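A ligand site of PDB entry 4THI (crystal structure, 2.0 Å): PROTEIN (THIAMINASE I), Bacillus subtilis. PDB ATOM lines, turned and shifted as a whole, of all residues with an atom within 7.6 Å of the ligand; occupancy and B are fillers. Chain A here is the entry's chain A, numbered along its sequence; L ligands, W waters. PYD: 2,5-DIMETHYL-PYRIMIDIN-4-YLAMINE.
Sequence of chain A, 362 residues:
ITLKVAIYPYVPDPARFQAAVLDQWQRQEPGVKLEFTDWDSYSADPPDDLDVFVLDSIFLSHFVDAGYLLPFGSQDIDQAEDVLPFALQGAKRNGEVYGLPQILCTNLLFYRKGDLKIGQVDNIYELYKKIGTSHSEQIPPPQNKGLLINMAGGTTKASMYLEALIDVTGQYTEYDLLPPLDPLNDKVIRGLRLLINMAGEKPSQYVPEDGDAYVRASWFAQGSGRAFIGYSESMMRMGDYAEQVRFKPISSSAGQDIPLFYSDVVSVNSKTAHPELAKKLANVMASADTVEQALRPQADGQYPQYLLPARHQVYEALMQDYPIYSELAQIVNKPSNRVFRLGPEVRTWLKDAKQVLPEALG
Merely in contact with the ligand: Tyr 8, Tyr 231, Glu 233, Tyr 262 and Asp 264. Of the 24 residues printed, 7 come within 4 Å of the ligand. The nearest printed residue that does not touch the ligand is Leu 307 (4.1 Å).
C6' of the ligand is covalently linked to SG of Cys 105 (1.8 Å). A nitrogen (N4') of the ligand sits at hydrogen-bond distance from the backbone carbonyl oxygen (O) of Tyr 10, 2.9 Å away.
O of Tyr 262 is in hydrogen-bond range of N of Cys 105 (3.0 Å). The side-chain amide nitrogen of Asn 107 lies close to the backbone NH of Tyr 231 (3.4 Å). O of Ile 103 is in hydrogen-bond range of N of Asp 264 (2.8 Å).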
ATOM      1  N   TYR A   8     -21.513 -13.035   6.030  1.00  0.00           N
ATOM      2  CA  TYR A   8     -21.640 -13.852   4.823  1.00  0.00           C
ATOM      3  C   TYR A   8     -22.433 -15.105   5.194  1.00  0.00           C
ATOM      4  O   TYR A   8     -22.030 -15.865   6.071  1.00  0.00           O
ATOM      5  CB  TYR A   8     -20.288 -14.217   4.231  1.00  0.00           C
ATOM      6  CG  TYR A   8     -20.409 -14.641   2.790  1.00  0.00           C
ATOM      7  CD1 TYR A   8     -20.743 -13.706   1.815  1.00  0.00           C
ATOM      8  CD2 TYR A   8     -20.267 -15.978   2.409  1.00  0.00           C
ATOM      9  CE1 TYR A   8     -20.932 -14.088   0.495  1.00  0.00           C
ATOM     10  CE2 TYR A   8     -20.458 -16.371   1.071  1.00  0.00           C
ATOM     11  CZ  TYR A   8     -20.797 -15.405   0.126  1.00  0.00           C
ATOM     12  OH  TYR A   8     -21.030 -15.746  -1.182  1.00  0.00           O
ATOM     13  N   PRO A   9     -23.563 -15.347   4.522  1.00  0.00           N
ATOM     14  CA  PRO A   9     -24.414 -16.500   4.802  1.00  0.00           C
ATOM     15  C   PRO A   9     -23.926 -17.892   4.440  1.00  0.00           C
ATOM     16  O   PRO A   9     -24.250 -18.857   5.143  1.00  0.00           O
ATOM     17  CB  PRO A   9     -25.709 -16.146   4.068  1.00  0.00           C
ATOM     18  CG  PRO A   9     -25.206 -15.418   2.864  1.00  0.00           C
ATOM     19  CD  PRO A   9     -24.136 -14.513   3.450  1.00  0.00           C
ATOM     20  N   TYR A  10     -23.118 -18.014   3.383  1.00  0.00           N
ATOM     21  CA  TYR A  10     -22.665 -19.335   2.969  1.00  0.00           C
ATOM     22  C   TYR A  10     -21.308 -19.837   3.484  1.00  0.00           C
ATOM     23  O   TYR A  10     -20.326 -19.888   2.744  1.00  0.00           O
ATOM     24  CB  TYR A  10     -22.742 -19.443   1.454  1.00  0.00           C
ATOM     25  CG  TYR A  10     -24.119 -19.093   0.937  1.00  0.00           C
ATOM     26  CD1 TYR A  10     -25.260 -19.629   1.536  1.00  0.00           C
ATOM     27  CD2 TYR A  10     -24.286 -18.217  -0.131  1.00  0.00           C
ATOM     28  CE1 TYR A  10     -26.543 -19.295   1.105  1.00  0.00           C
ATOM     29  CE2 TYR A  10     -25.556 -17.879  -0.590  1.00  0.00           C
ATOM     30  CZ  TYR A  10     -26.681 -18.425   0.038  1.00  0.00           C
ATOM     31  OH  TYR A  10     -27.950 -18.075  -0.382  1.00  0.00           O
ATOM     32  N   VAL A  11     -21.291 -20.242   4.761  1.00  0.00           N
ATOM     33  CA  VAL A  11     -20.092 -20.788   5.419  1.00  0.00           C
ATOM     34  C   VAL A  11     -20.550 -21.997   6.241  1.00  0.00           C
ATOM     35  O   VAL A  11     -21.744 -22.149   6.511  1.00  0.00           O
ATOM     36  CB  VAL A  11     -19.420 -19.748   6.372  1.00  0.00           C
ATOM     37  CG1 VAL A  11     -18.833 -18.603   5.591  1.00  0.00           C
ATOM     38  CG2 VAL A  11     -20.424 -19.227   7.405  1.00  0.00           C
ATOM     39  N   PRO A  12     -19.608 -22.884   6.618  1.00  0.00           N
ATOM     40  CA  PRO A  12     -19.940 -24.079   7.411  1.00  0.00           C
ATOM     41  C   PRO A  12     -20.691 -23.767   8.702  1.00  0.00           C
ATOM     42  O   PRO A  12     -21.589 -24.514   9.083  1.00  0.00           O
ATOM     43  CB  PRO A  12     -18.575 -24.703   7.671  1.00  0.00           C
ATOM     44  CG  PRO A  12     -17.849 -24.414   6.398  1.00  0.00           C
ATOM     45  CD  PRO A  12     -18.195 -22.958   6.175  1.00  0.00           C
ATOM     46  N   TYR A  42     -26.060 -12.930  -4.078  1.00  0.00           N
ATOM     47  CA  TYR A  42     -26.347 -13.683  -5.300  1.00  0.00           C
ATOM     48  C   TYR A  42     -27.779 -13.503  -5.804  1.00  0.00           C
ATOM     49  O   TYR A  42     -28.035 -13.676  -7.000  1.00  0.00           O
ATOM     50  CB  TYR A  42     -26.080 -15.185  -5.102  1.00  0.00           C
ATOM     51  CG  TYR A  42     -24.651 -15.598  -5.333  1.00  0.00           C
ATOM     52  CD1 TYR A  42     -24.217 -15.959  -6.606  1.00  0.00           C
ATOM     53  CD2 TYR A  42     -23.730 -15.652  -4.283  1.00  0.00           C
ATOM     54  CE1 TYR A  42     -22.888 -16.356  -6.828  1.00  0.00           C
ATOM     55  CE2 TYR A  42     -22.411 -16.050  -4.491  1.00  0.00           C
ATOM     56  CZ  TYR A  42     -21.994 -16.395  -5.762  1.00  0.00           C
ATOM     57  OH  TYR A  42     -20.692 -16.777  -5.990  1.00  0.00           O
ATOM     58  N   ASP A  56     -20.084 -11.357  -2.379  1.00  0.00           N
ATOM     59  CA  ASP A  56     -19.143 -12.064  -3.251  1.00  0.00           C
ATOM     60  C   ASP A  56     -18.746 -11.007  -4.304  1.00  0.00           C
ATOM     61  O   ASP A  56     -19.619 -10.405  -4.948  1.00  0.00           O
ATOM     62  CB  ASP A  56     -19.826 -13.254  -3.927  1.00  0.00           C
ATOM     63  CG  ASP A  56     -18.874 -14.098  -4.765  1.00  0.00           C
ATOM     64  OD1 ASP A  56     -18.134 -13.537  -5.607  1.00  0.00           O
ATOM     65  OD2 ASP A  56     -18.878 -15.330  -4.615  1.00  0.00           O
ATOM     66  N   ILE A 103     -13.012 -13.209   3.351  1.00  0.00           N
ATOM     67  CA  ILE A 103     -12.860 -14.635   3.046  1.00  0.00           C
ATOM     68  C   ILE A 103     -12.525 -14.823   1.571  1.00  0.00           C
ATOM     69  O   ILE A 103     -12.992 -14.065   0.746  1.00  0.00           O
ATOM     70  CB  ILE A 103     -14.178 -15.417   3.314  1.00  0.00           C
ATOM     71  CG1 ILE A 103     -14.634 -15.224   4.771  1.00  0.00           C
ATOM     72  CG2 ILE A 103     -13.990 -16.919   2.993  1.00  0.00           C
ATOM     73  CD1 ILE A 103     -16.094 -15.548   4.976  1.00  0.00           C
ATOM     74  N   LEU A 104     -11.688 -15.822   1.277  1.00  0.00           N
ATOM     75  CA  LEU A 104     -11.287 -16.166  -0.097  1.00  0.00           C
ATOM     76  C   LEU A 104     -11.647 -17.635  -0.329  1.00  0.00           C
ATOM     77  O   LEU A 104     -11.659 -18.414   0.637  1.00  0.00           O
ATOM     78  CB  LEU A 104      -9.788 -15.955  -0.296  1.00  0.00           C
ATOM     79  CG  LEU A 104      -9.262 -14.515  -0.246  1.00  0.00           C
ATOM     80  CD1 LEU A 104      -7.760 -14.551  -0.007  1.00  0.00           C
ATOM     81  CD2 LEU A 104      -9.583 -13.795  -1.548  1.00  0.00           C
ATOM     82  N   CYS A 105     -11.897 -18.000  -1.586  1.00  0.00           N
ATOM     83  CA  CYS A 105     -12.286 -19.379  -1.915  1.00  0.00           C
ATOM     84  C   CYS A 105     -11.722 -19.871  -3.237  1.00  0.00           C
ATOM     85  O   CYS A 105     -11.622 -19.119  -4.216  1.00  0.00           O
ATOM     86  CB  CYS A 105     -13.807 -19.463  -2.024  1.00  0.00           C
ATOM     87  SG  CYS A 105     -14.841 -18.959  -0.640  1.00  0.00           S
ATOM     88  N   THR A 106     -11.423 -21.165  -3.294  1.00  0.00           N
ATOM     89  CA  THR A 106     -10.914 -21.811  -4.497  1.00  0.00           C
ATOM     90  C   THR A 106     -11.155 -23.330  -4.416  1.00  0.00           C
ATOM     91  O   THR A 106     -11.151 -23.893  -3.324  1.00  0.00           O
ATOM     92  CB  THR A 106      -9.383 -21.545  -4.730  1.00  0.00           C
ATOM     93  OG1 THR A 106      -9.039 -22.015  -6.038  1.00  0.00           O
ATOM     94  CG2 THR A 106      -8.494 -22.245  -3.714  1.00  0.00           C
ATOM     95  N   ASN A 107     -11.474 -23.960  -5.545  1.00  0.00           N
ATOM     96  CA  ASN A 107     -11.666 -25.410  -5.567  1.00  0.00           C
ATOM     97  C   ASN A 107     -10.247 -26.005  -5.455  1.00  0.00           C
ATOM     98  O   ASN A 107      -9.280 -25.391  -5.913  1.00  0.00           O
ATOM     99  CB  ASN A 107     -12.315 -25.896  -6.874  1.00  0.00           C
ATOM    100  CG  ASN A 107     -13.856 -25.941  -6.829  1.00  0.00           C
ATOM    101  OD1 ASN A 107     -14.511 -25.714  -7.850  1.00  0.00           O
ATOM    102  ND2 ASN A 107     -14.420 -26.266  -5.674  1.00  0.00           N
ATOM    103  N   THR A 156     -23.228 -21.313 -10.967  1.00  0.00           N
ATOM    104  CA  THR A 156     -22.002 -22.073 -10.708  1.00  0.00           C
ATOM    105  C   THR A 156     -21.352 -22.440 -12.029  1.00  0.00           C
ATOM    106  O   THR A 156     -20.153 -22.245 -12.208  1.00  0.00           O
ATOM    107  CB  THR A 156     -22.278 -23.353  -9.916  1.00  0.00           C
ATOM    108  OG1 THR A 156     -22.615 -22.996  -8.577  1.00  0.00           O
ATOM    109  CG2 THR A 156     -21.048 -24.245  -9.871  1.00  0.00           C
ATOM    110  N   SER A 159     -20.141 -19.313 -13.731  1.00  0.00           N
ATOM    111  CA  SER A 159     -18.902 -18.880 -13.075  1.00  0.00           C
ATOM    112  C   SER A 159     -17.718 -19.718 -13.584  1.00  0.00           C
ATOM    113  O   SER A 159     -16.657 -19.169 -13.917  1.00  0.00           O
ATOM    114  CB  SER A 159     -19.009 -19.027 -11.558  1.00  0.00           C
ATOM    115  OG  SER A 159     -19.908 -18.084 -11.028  1.00  0.00           O
ATOM    116  N   ALA A 213     -24.747 -27.878   1.694  1.00  0.00           N
ATOM    117  CA  ALA A 213     -23.710 -27.546   0.723  1.00  0.00           C
ATOM    118  C   ALA A 213     -22.428 -28.365   0.849  1.00  0.00           C
ATOM    119  O   ALA A 213     -21.589 -28.349  -0.049  1.00  0.00           O
ATOM    120  CB  ALA A 213     -23.400 -26.057   0.794  1.00  0.00           C
ATOM    121  N   TYR A 214     -22.294 -29.100   1.940  1.00  0.00           N
ATOM    122  CA  TYR A 214     -21.085 -29.901   2.166  1.00  0.00           C
ATOM    123  C   TYR A 214     -21.294 -31.431   2.181  1.00  0.00           C
ATOM    124  O   TYR A 214     -20.464 -32.174   2.715  1.00  0.00           O
ATOM    125  CB  TYR A 214     -20.396 -29.429   3.444  1.00  0.00           C
ATOM    126  CG  TYR A 214     -20.203 -27.920   3.466  1.00  0.00           C
ATOM    127  CD1 TYR A 214     -19.308 -27.306   2.593  1.00  0.00           C
ATOM    128  CD2 TYR A 214     -20.958 -27.107   4.307  1.00  0.00           C
ATOM    129  CE1 TYR A 214     -19.177 -25.923   2.542  1.00  0.00           C
ATOM    130  CE2 TYR A 214     -20.835 -25.716   4.265  1.00  0.00           C
ATOM    131  CZ  TYR A 214     -19.947 -25.134   3.376  1.00  0.00           C
ATOM    132  OH  TYR A 214     -19.835 -23.749   3.302  1.00  0.00           O
ATOM    133  N   TYR A 231     -14.226 -26.802  -2.339  1.00  0.00           N
ATOM    134  CA  TYR A 231     -13.584 -25.709  -1.602  1.00  0.00           C
ATOM    135  C   TYR A 231     -12.831 -26.214  -0.377  1.00  0.00           C
ATOM    136  O   TYR A 231     -13.091 -27.330   0.084  1.00  0.00           O
ATOM    137  CB  TYR A 231     -14.634 -24.672  -1.187  1.00  0.00           C
ATOM    138  CG  TYR A 231     -15.345 -24.043  -2.372  1.00  0.00           C
ATOM    139  CD1 TYR A 231     -14.623 -23.581  -3.480  1.00  0.00           C
ATOM    140  CD2 TYR A 231     -16.741 -23.940  -2.402  1.00  0.00           C
ATOM    141  CE1 TYR A 231     -15.271 -23.028  -4.589  1.00  0.00           C
ATOM    142  CE2 TYR A 231     -17.401 -23.399  -3.516  1.00  0.00           C
ATOM    143  CZ  TYR A 231     -16.660 -22.938  -4.600  1.00  0.00           C
ATOM    144  OH  TYR A 231     -17.282 -22.408  -5.698  1.00  0.00           O
ATOM    145  N   GLU A 233     -13.143 -25.294   2.677  1.00  0.00           N
ATOM    146  CA  GLU A 233     -14.100 -25.448   3.793  1.00  0.00           C
ATOM    147  C   GLU A 233     -14.706 -26.846   3.899  1.00  0.00           C
ATOM    148  O   GLU A 233     -15.320 -27.190   4.928  1.00  0.00           O
ATOM    149  CB  GLU A 233     -15.280 -24.464   3.702  1.00  0.00           C
ATOM    150  CG  GLU A 233     -14.939 -23.074   3.329  1.00  0.00           C
ATOM    151  CD  GLU A 233     -14.883 -22.865   1.837  1.00  0.00           C
ATOM    152  OE1 GLU A 233     -15.948 -22.829   1.193  1.00  0.00           O
ATOM    153  OE2 GLU A 233     -13.757 -22.704   1.321  1.00  0.00           O
ATOM    154  N   PHE A 261      -9.537 -16.511  -7.444  1.00  0.00           N
ATOM    155  CA  PHE A 261     -10.163 -16.699  -6.144  1.00  0.00           C
ATOM    156  C   PHE A 261     -11.449 -15.889  -5.973  1.00  0.00           C
ATOM    157  O   PHE A 261     -11.500 -14.721  -6.326  1.00  0.00           O
ATOM    158  CB  PHE A 261      -9.204 -16.238  -5.019  1.00  0.00           C
ATOM    159  CG  PHE A 261      -8.025 -17.143  -4.799  1.00  0.00           C
ATOM    160  CD1 PHE A 261      -7.009 -17.220  -5.725  1.00  0.00           C
ATOM    161  CD2 PHE A 261      -7.970 -17.956  -3.668  1.00  0.00           C
ATOM    162  CE1 PHE A 261      -5.946 -18.100  -5.546  1.00  0.00           C
ATOM    163  CE2 PHE A 261      -6.917 -18.837  -3.476  1.00  0.00           C
ATOM    164  CZ  PHE A 261      -5.900 -18.911  -4.415  1.00  0.00           C
ATOM    165  N   TYR A 262     -12.484 -16.509  -5.414  1.00  0.00           N
ATOM    166  CA  TYR A 262     -13.712 -15.782  -5.104  1.00  0.00           C
ATOM    167  C   TYR A 262     -13.347 -14.990  -3.830  1.00  0.00           C
ATOM    168  O   TYR A 262     -12.627 -15.489  -2.956  1.00  0.00           O
ATOM    169  CB  TYR A 262     -14.855 -16.751  -4.784  1.00  0.00           C
ATOM    170  CG  TYR A 262     -15.383 -17.525  -5.952  1.00  0.00           C
ATOM    171  CD1 TYR A 262     -16.422 -17.020  -6.737  1.00  0.00           C
ATOM    172  CD2 TYR A 262     -14.870 -18.777  -6.271  1.00  0.00           C
ATOM    173  CE1 TYR A 262     -16.935 -17.750  -7.828  1.00  0.00           C
ATOM    174  CE2 TYR A 262     -15.375 -19.517  -7.356  1.00  0.00           C
ATOM    175  CZ  TYR A 262     -16.401 -18.990  -8.120  1.00  0.00           C
ATOM    176  OH  TYR A 262     -16.881 -19.703  -9.189  1.00  0.00           O
ATOM    177  N   SER A 263     -13.812 -13.751  -3.729  1.00  0.00           N
ATOM    178  CA  SER A 263     -13.490 -12.936  -2.569  1.00  0.00           C
ATOM    179  C   SER A 263     -14.718 -12.297  -1.952  1.00  0.00           C
ATOM    180  O   SER A 263     -15.426 -11.537  -2.609  1.00  0.00           O
ATOM    181  CB  SER A 263     -12.484 -11.848  -2.939  1.00  0.00           C
ATOM    182  OG  SER A 263     -12.158 -11.073  -1.803  1.00  0.00           O
ATOM    183  N   ASP A 264     -14.972 -12.631  -0.697  1.00  0.00           N
ATOM    184  CA  ASP A 264     -16.122 -12.095   0.012  1.00  0.00           C
ATOM    185  C   ASP A 264     -15.630 -10.869   0.774  1.00  0.00           C
ATOM    186  O   ASP A 264     -14.797 -10.995   1.674  1.00  0.00           O
ATOM    187  CB  ASP A 264     -16.720 -13.158   0.943  1.00  0.00           C
ATOM    188  CG  ASP A 264     -16.991 -14.500   0.210  1.00  0.00           C
ATOM    189  OD1 ASP A 264     -17.370 -14.464  -0.984  1.00  0.00           O
ATOM    190  OD2 ASP A 264     -16.822 -15.581   0.806  1.00  0.00           O
ATOM    191  N   LEU A 307     -12.000 -22.245   6.272  1.00  0.00           N
ATOM    192  CA  LEU A 307     -12.204 -21.166   5.307  1.00  0.00           C
ATOM    193  C   LEU A 307     -10.854 -20.456   5.149  1.00  0.00           C
ATOM    194  O   LEU A 307     -10.064 -20.428   6.089  1.00  0.00           O
ATOM    195  CB  LEU A 307     -13.227 -20.175   5.853  1.00  0.00           C
ATOM    196  CG  LEU A 307     -14.696 -20.577   5.906  1.00  0.00           C
ATOM    197  CD1 LEU A 307     -15.414 -19.787   6.957  1.00  0.00           C
ATOM    198  CD2 LEU A 307     -15.328 -20.311   4.547  1.00  0.00           C
ATOM    199  N   LEU A 308     -10.621 -19.845   3.988  1.00  0.00           N
ATOM    200  CA  LEU A 308      -9.365 -19.119   3.722  1.00  0.00           C
ATOM    201  C   LEU A 308      -9.438 -17.645   4.098  1.00  0.00           C
ATOM    202  O   LEU A 308     -10.222 -16.883   3.515  1.00  0.00           O
ATOM    203  CB  LEU A 308      -9.024 -19.177   2.228  1.00  0.00           C
ATOM    204  CG  LEU A 308      -8.846 -20.548   1.573  1.00  0.00           C
ATOM    205  CD1 LEU A 308      -8.673 -20.372   0.069  1.00  0.00           C
ATOM    206  CD2 LEU A 308      -7.657 -21.265   2.182  1.00  0.00           C
HETATM  207  N1' PYD L   1     -16.736 -19.442  -2.594  1.00  0.00           N
HETATM  208  C2' PYD L   1     -17.986 -19.681  -3.072  1.00  0.00           C
HETATM  209  CM2 PYD L   1     -18.131 -19.811  -4.511  1.00  0.00           C
HETATM  210  N3' PYD L   1     -19.033 -19.795  -2.276  1.00  0.00           N
HETATM  211  C4' PYD L   1     -18.841 -19.653  -0.918  1.00  0.00           C
HETATM  212  N4' PYD L   1     -19.897 -19.769  -0.166  1.00  0.00           N
HETATM  213  C5' PYD L   1     -17.547 -19.376  -0.360  1.00  0.00           C
HETATM  214  C6' PYD L   1     -16.521 -19.292  -1.253  1.00  0.00           C
HETATM  215  C7' PYD L   1     -17.315 -19.208   1.132  1.00  0.00           C
HETATM  216  O   HOH W   1     -18.462 -16.686  -2.289  1.00  0.00           O
